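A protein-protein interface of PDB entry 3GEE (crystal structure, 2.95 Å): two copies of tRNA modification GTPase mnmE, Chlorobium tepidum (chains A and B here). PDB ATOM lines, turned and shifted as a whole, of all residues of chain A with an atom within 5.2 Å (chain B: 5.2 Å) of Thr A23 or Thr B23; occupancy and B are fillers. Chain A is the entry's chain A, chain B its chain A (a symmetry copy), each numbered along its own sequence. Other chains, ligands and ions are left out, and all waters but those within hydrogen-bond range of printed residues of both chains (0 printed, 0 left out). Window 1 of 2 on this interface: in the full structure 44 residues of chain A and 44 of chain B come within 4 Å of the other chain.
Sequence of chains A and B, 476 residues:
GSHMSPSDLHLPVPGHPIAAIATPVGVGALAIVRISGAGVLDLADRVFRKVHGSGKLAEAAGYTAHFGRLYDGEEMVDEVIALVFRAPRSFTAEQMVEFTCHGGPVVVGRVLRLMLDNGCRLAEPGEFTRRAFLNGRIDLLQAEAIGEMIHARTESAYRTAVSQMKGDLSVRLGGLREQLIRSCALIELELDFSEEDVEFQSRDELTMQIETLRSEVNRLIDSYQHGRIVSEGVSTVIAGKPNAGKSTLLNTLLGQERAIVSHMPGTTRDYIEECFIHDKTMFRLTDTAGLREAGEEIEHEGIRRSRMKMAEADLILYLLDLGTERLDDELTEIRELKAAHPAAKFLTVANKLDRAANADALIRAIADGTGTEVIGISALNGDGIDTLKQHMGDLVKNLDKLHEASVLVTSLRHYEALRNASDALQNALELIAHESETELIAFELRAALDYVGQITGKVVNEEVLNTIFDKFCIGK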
ATOM      1  N   ILE A  21     -30.312  31.651  18.237  1.00  0.00           N
ATOM      2  CA  ILE A  21     -30.280  31.261  19.641  1.00  0.00           C
ATOM      3  C   ILE A  21     -29.877  29.799  19.616  1.00  0.00           C
ATOM      4  O   ILE A  21     -30.465  29.018  18.876  1.00  0.00           O
ATOM      5  CB  ILE A  21     -31.681  31.363  20.278  1.00  0.00           C
ATOM      6  CG1 ILE A  21     -32.419  32.633  19.805  1.00  0.00           C
ATOM      7  CG2 ILE A  21     -31.606  31.217  21.780  1.00  0.00           C
ATOM      8  CD1 ILE A  21     -32.423  33.797  20.768  1.00  0.00           C
ATOM      9  N   ALA A  22     -28.867  29.423  20.394  1.00  0.00           N
ATOM     10  CA  ALA A  22     -28.303  28.073  20.297  1.00  0.00           C
ATOM     11  C   ALA A  22     -28.679  27.203  21.486  1.00  0.00           C
ATOM     12  O   ALA A  22     -28.497  25.981  21.465  1.00  0.00           O
ATOM     13  CB  ALA A  22     -26.794  28.140  20.140  1.00  0.00           C
ATOM     14  N   THR A  23     -29.202  27.854  22.519  1.00  0.00           N
ATOM     15  CA  THR A  23     -29.604  27.204  23.762  1.00  0.00           C
ATOM     16  C   THR A  23     -31.126  26.999  23.813  1.00  0.00           C
ATOM     17  O   THR A  23     -31.857  27.642  23.057  1.00  0.00           O
ATOM     18  CB  THR A  23     -29.157  28.058  24.944  1.00  0.00           C
ATOM     19  OG1 THR A  23     -29.535  29.425  24.708  1.00  0.00           O
ATOM     20  CG2 THR A  23     -27.650  27.968  25.089  1.00  0.00           C
ATOM     21  N   PRO A  24     -31.611  26.099  24.692  1.00  0.00           N
ATOM     22  CA  PRO A  24     -33.049  25.830  24.756  1.00  0.00           C
ATOM     23  C   PRO A  24     -33.844  27.062  25.151  1.00  0.00           C
ATOM     24  O   PRO A  24     -33.356  27.898  25.902  1.00  0.00           O
ATOM     25  CB  PRO A  24     -33.166  24.772  25.858  1.00  0.00           C
ATOM     26  CG  PRO A  24     -31.841  24.147  25.929  1.00  0.00           C
ATOM     27  CD  PRO A  24     -30.874  25.270  25.660  1.00  0.00           C
ATOM     28  N   VAL A  25     -35.062  27.162  24.635  1.00  0.00           N
ATOM     29  CA  VAL A  25     -35.979  28.242  24.982  1.00  0.00           C
ATOM     30  C   VAL A  25     -36.245  28.238  26.485  1.00  0.00           C
ATOM     31  O   VAL A  25     -36.364  27.172  27.099  1.00  0.00           O
ATOM     32  CB  VAL A  25     -37.331  28.080  24.248  1.00  0.00           C
ATOM     33  CG1 VAL A  25     -38.134  29.375  24.313  1.00  0.00           C
ATOM     34  CG2 VAL A  25     -37.107  27.663  22.798  1.00  0.00           C
ATOM     35  N   VAL A  27     -35.980  30.109  30.637  1.00  0.00           N
ATOM     36  CA  VAL A  27     -35.354  30.941  31.638  1.00  0.00           C
ATOM     37  C   VAL A  27     -34.166  30.202  32.219  1.00  0.00           C
ATOM     38  O   VAL A  27     -34.291  29.066  32.691  1.00  0.00           O
ATOM     39  CB  VAL A  27     -36.368  31.331  32.737  1.00  0.00           C
ATOM     40  CG1 VAL A  27     -35.676  31.936  33.940  1.00  0.00           C
ATOM     41  CG2 VAL A  27     -37.392  32.304  32.184  1.00  0.00           C
ATOM     42  N   GLY A  28     -33.009  30.853  32.163  1.00  0.00           N
ATOM     43  CA  GLY A  28     -31.788  30.312  32.744  1.00  0.00           C
ATOM     44  C   GLY A  28     -30.788  31.393  33.093  1.00  0.00           C
ATOM     45  O   GLY A  28     -31.006  32.574  32.809  1.00  0.00           O
ATOM     46  N   ALA A  29     -29.687  30.983  33.717  1.00  0.00           N
ATOM     47  CA  ALA A  29     -28.579  31.883  33.993  1.00  0.00           C
ATOM     48  C   ALA A  29     -27.972  32.429  32.702  1.00  0.00           C
ATOM     49  O   ALA A  29     -27.713  33.625  32.589  1.00  0.00           O
ATOM     50  CB  ALA A  29     -27.533  31.179  34.802  1.00  0.00           C
ATOM     51  N   LEU A  30     -27.755  31.563  31.721  1.00  0.00           N
ATOM     52  CA  LEU A  30     -27.053  31.978  30.523  1.00  0.00           C
ATOM     53  C   LEU A  30     -27.700  31.440  29.274  1.00  0.00           C
ATOM     54  O   LEU A  30     -28.340  30.393  29.308  1.00  0.00           O
ATOM     55  CB  LEU A  30     -25.607  31.483  30.562  1.00  0.00           C
ATOM     56  CG  LEU A  30     -24.719  31.806  31.755  1.00  0.00           C
ATOM     57  CD1 LEU A  30     -23.477  30.975  31.640  1.00  0.00           C
ATOM     58  CD2 LEU A  30     -24.399  33.283  31.805  1.00  0.00           C
ATOM     59  N   ALA A  31     -27.504  32.155  28.171  1.00  0.00           N
ATOM     60  CA  ALA A  31     -27.910  31.713  26.845  1.00  0.00           C
ATOM     61  C   ALA A  31     -26.771  31.990  25.863  1.00  0.00           C
ATOM     62  O   ALA A  31     -25.906  32.822  26.136  1.00  0.00           O
ATOM     63  CB  ALA A  31     -29.146  32.455  26.420  1.00  0.00           C
ATOM     64  N   ILE A  32     -26.786  31.311  24.718  1.00  0.00           N
ATOM     65  CA  ILE A  32     -25.784  31.508  23.676  1.00  0.00           C
ATOM     66  C   ILE A  32     -26.442  31.889  22.348  1.00  0.00           C
ATOM     67  O   ILE A  32     -27.196  31.097  21.773  1.00  0.00           O
ATOM     68  CB  ILE A  32     -24.960  30.221  23.427  1.00  0.00           C
ATOM     69  CG1 ILE A  32     -24.241  29.764  24.693  1.00  0.00           C
ATOM     70  CG2 ILE A  32     -23.968  30.419  22.279  1.00  0.00           C
ATOM     71  CD1 ILE A  32     -23.815  28.311  24.636  1.00  0.00           C
ATOM     72  N   ILE B  21     -26.087  23.223  35.729  1.00  0.00           N
ATOM     73  CA  ILE B  21     -26.554  23.503  34.377  1.00  0.00           C
ATOM     74  C   ILE B  21     -26.894  24.981  34.394  1.00  0.00           C
ATOM     75  O   ILE B  21     -27.602  25.431  35.288  1.00  0.00           O
ATOM     76  CB  ILE B  21     -27.842  22.716  34.059  1.00  0.00           C
ATOM     77  CG1 ILE B  21     -27.768  21.277  34.611  1.00  0.00           C
ATOM     78  CG2 ILE B  21     -28.178  22.795  32.588  1.00  0.00           C
ATOM     79  CD1 ILE B  21     -27.434  20.196  33.609  1.00  0.00           C
ATOM     80  N   ALA B  22     -26.381  25.744  33.435  1.00  0.00           N
ATOM     81  CA  ALA B  22     -26.515  27.204  33.482  1.00  0.00           C
ATOM     82  C   ALA B  22     -27.509  27.725  32.455  1.00  0.00           C
ATOM     83  O   ALA B  22     -27.925  28.888  32.504  1.00  0.00           O
ATOM     84  CB  ALA B  22     -25.161  27.866  33.298  1.00  0.00           C
ATOM     85  N   THR B  23     -27.875  26.848  31.528  1.00  0.00           N
ATOM     86  CA  THR B  23     -28.799  27.160  30.442  1.00  0.00           C
ATOM     87  C   THR B  23     -30.206  26.619  30.739  1.00  0.00           C
ATOM     88  O   THR B  23     -30.361  25.751  31.600  1.00  0.00           O
ATOM     89  CB  THR B  23     -28.274  26.553  29.145  1.00  0.00           C
ATOM     90  OG1 THR B  23     -27.900  25.185  29.381  1.00  0.00           O
ATOM     91  CG2 THR B  23     -27.063  27.336  28.677  1.00  0.00           C
ATOM     92  N   PRO B  24     -31.239  27.133  30.041  1.00  0.00           N
ATOM     93  CA  PRO B  24     -32.607  26.687  30.310  1.00  0.00           C
ATOM     94  C   PRO B  24     -32.791  25.206  30.032  1.00  0.00           C
ATOM     95  O   PRO B  24     -32.145  24.659  29.146  1.00  0.00           O
ATOM     96  CB  PRO B  24     -33.449  27.501  29.322  1.00  0.00           C
ATOM     97  CG  PRO B  24     -32.628  28.672  28.996  1.00  0.00           C
ATOM     98  CD  PRO B  24     -31.215  28.156  28.982  1.00  0.00           C
ATOM     99  N   VAL B  25     -33.670  24.573  30.796  1.00  0.00           N
ATOM    100  CA  VAL B  25     -34.020  23.169  30.600  1.00  0.00           C
ATOM    101  C   VAL B  25     -34.580  22.964  29.196  1.00  0.00           C
ATOM    102  O   VAL B  25     -35.320  23.810  28.683  1.00  0.00           O
ATOM    103  CB  VAL B  25     -35.088  22.715  31.622  1.00  0.00           C
ATOM    104  CG1 VAL B  25     -35.177  21.193  31.663  1.00  0.00           C
ATOM    105  CG2 VAL B  25     -34.775  23.270  33.008  1.00  0.00           C
ATOM    106  N   VAL B  27     -34.385  21.210  24.989  1.00  0.00           N
ATOM    107  CA  VAL B  27     -33.678  20.717  23.829  1.00  0.00           C
ATOM    108  C   VAL B  27     -33.141  21.895  23.043  1.00  0.00           C
ATOM    109  O   VAL B  27     -33.888  22.809  22.675  1.00  0.00           O
ATOM    110  CB  VAL B  27     -34.603  19.833  22.960  1.00  0.00           C
ATOM    111  CG1 VAL B  27     -33.991  19.560  21.603  1.00  0.00           C
ATOM    112  CG2 VAL B  27     -34.895  18.525  23.670  1.00  0.00           C
ATOM    113  N   GLY B  28     -31.834  21.872  22.806  1.00  0.00           N
ATOM    114  CA  GLY B  28     -31.175  22.891  22.002  1.00  0.00           C
ATOM    115  C   GLY B  28     -29.888  22.392  21.381  1.00  0.00           C
ATOM    116  O   GLY B  28     -29.454  21.266  21.640  1.00  0.00           O
ATOM    117  N   ALA B  29     -29.279  23.238  20.554  1.00  0.00           N
ATOM    118  CA  ALA B  29     -27.969  22.953  19.991  1.00  0.00           C
ATOM    119  C   ALA B  29     -26.908  22.832  21.084  1.00  0.00           C
ATOM    120  O   ALA B  29     -26.099  21.908  21.069  1.00  0.00           O
ATOM    121  CB  ALA B  29     -27.586  24.021  19.012  1.00  0.00           C
ATOM    122  N   LEU B  30     -26.917  23.751  22.040  1.00  0.00           N
ATOM    123  CA  LEU B  30     -25.857  23.784  23.029  1.00  0.00           C
ATOM    124  C   LEU B  30     -26.389  24.023  24.418  1.00  0.00           C
ATOM    125  O   LEU B  30     -27.437  24.640  24.585  1.00  0.00           O
ATOM    126  CB  LEU B  30     -24.865  24.900  22.700  1.00  0.00           C
ATOM    127  CG  LEU B  30     -24.217  24.968  21.324  1.00  0.00           C
ATOM    128  CD1 LEU B  30     -23.524  26.292  21.210  1.00  0.00           C
ATOM    129  CD2 LEU B  30     -23.258  23.817  21.123  1.00  0.00           C
ATOM    130  N   ALA B  31     -25.641  23.548  25.408  1.00  0.00           N
ATOM    131  CA  ALA B  31     -25.904  23.820  26.813  1.00  0.00           C
ATOM    132  C   ALA B  31     -24.584  24.168  27.504  1.00  0.00           C
ATOM    133  O   ALA B  31     -23.514  23.829  27.001  1.00  0.00           O
ATOM    134  CB  ALA B  31     -26.516  22.607  27.459  1.00  0.00           C
ATOM    135  N   ILE B  32     -24.665  24.823  28.660  1.00  0.00           N
ATOM    136  CA  ILE B  32     -23.488  25.181  29.443  1.00  0.00           C
ATOM    137  C   ILE B  32     -23.577  24.610  30.860  1.00  0.00           C
ATOM    138  O   ILE B  32     -24.468  24.983  31.631  1.00  0.00           O
ATOM    139  CB  ILE B  32     -23.337  26.717  29.576  1.00  0.00           C
ATOM    140  CG1 ILE B  32     -23.218  27.386  28.211  1.00  0.00           C
ATOM    141  CG2 ILE B  32     -22.144  27.075  30.464  1.00  0.00           C
ATOM    142  CD1 ILE B  32     -23.527  28.869  28.254  1.00  0.00           C
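The backbone carbonyl oxygen of Ala A22 lies within hydrogen-bond range of the backbone NH of Leu B30.
N of Ala B29 sits at hydrogen-bond distance from O of Ala A22 (3.0 Å).
N of Leu A30 is in hydrogen-bond range of O of Ala B22 (2.8 Å).
The backbone NH (N) of Ala A29 sits at hydrogen-bond distance from the backbone carbonyl oxygen (O) of Ala B22 (3.0 Å).
The backbone NH (N) of Ala A22 sits at hydrogen-bond distance from the backbone carbonyl oxygen (O) of Ile A32, 2.7 Å away.
OG1 of Thr A23 is in hydrogen-bond range of N of Ile A32, 3.3 Å away.
OG1 of Thr B23 lies within hydrogen-bond range of N of Ile B32, 3.3 Å away.
The backbone carbonyl oxygen of Ile B32 sits at hydrogen-bond distance from the backbone NH of Ala B22 (2.7 Å).
Thr A23 touches Thr B23.
O of Leu B30 touches CG2 of Thr A23, at 3.4 Å.
Pro A24 touches Pro B24.
Pro A24 touches Val B25.
Pro A24 touches Val B27.
Gly B28 touches Pro A24.
Pro A24 touches Leu B30.
O of Ala B22 touches C of Gly A28 (3.8 Å).
CG2 of Thr B23 touches O of Leu A30, 3.4 Å away.
Ile A32 touches Leu B30.
Ile A21 touches none of the printed residues of chain B.
Printed residues of chain B within 4 Å of Thr A23: Thr B23 (3.7 Å) and Leu B30 (3.4 Å).
Printed residues of chain B within 4 Å of Val A27: Pro B24 (3.8 Å).
Ala A31 touches none of the printed residues of chain B.
Thr B23 touches two residues of chain A.
Printed residues of chain A within 4 Å of Val B25: Pro A24 and Val A25.
The nearest printed residue of chain B that does not touch Val A27 is Val B25 (4.9 Å).
Of the 11 printed residues of chain B, 9 touch a printed residue of chain A.
Hydrophobic or aromatic side chains of chain B within 4 Å of the printed part of chain A: Ala B22, Pro B24, Ala B29, Leu B30 and Ile B32.
Printed residues of chain A that touch a printed residue of chain B: Ala A22, Thr A23, Pro A24, Val A25, Val A27, Gly A28, Ala A29, Leu A30 and Ile A32.
Hydrophobic or aromatic side chains of chain A that line the printed part of chain B: Ala A22, Pro A24, Ala A29, Leu A30 and Ile A32.
Among the printed residues, 22 pairs touch across the chains.
Ala A22 touches Gly B28, and with the chains exchanged Gly A28 touches Ala B22.
Pro A24 touches Val B25, and with the chains exchanged Val A25 touches Pro B24.
Pro A24 touches Gly B28, and with the chains exchanged Gly A28 touches Pro B24.
Val A25 touches its own counterpart, Val B25.
11 positions are printed for both chains.
Of the 22 pairs that touch across the chains among the printed residues, 22 have their exchanged pair printed and touching as well.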
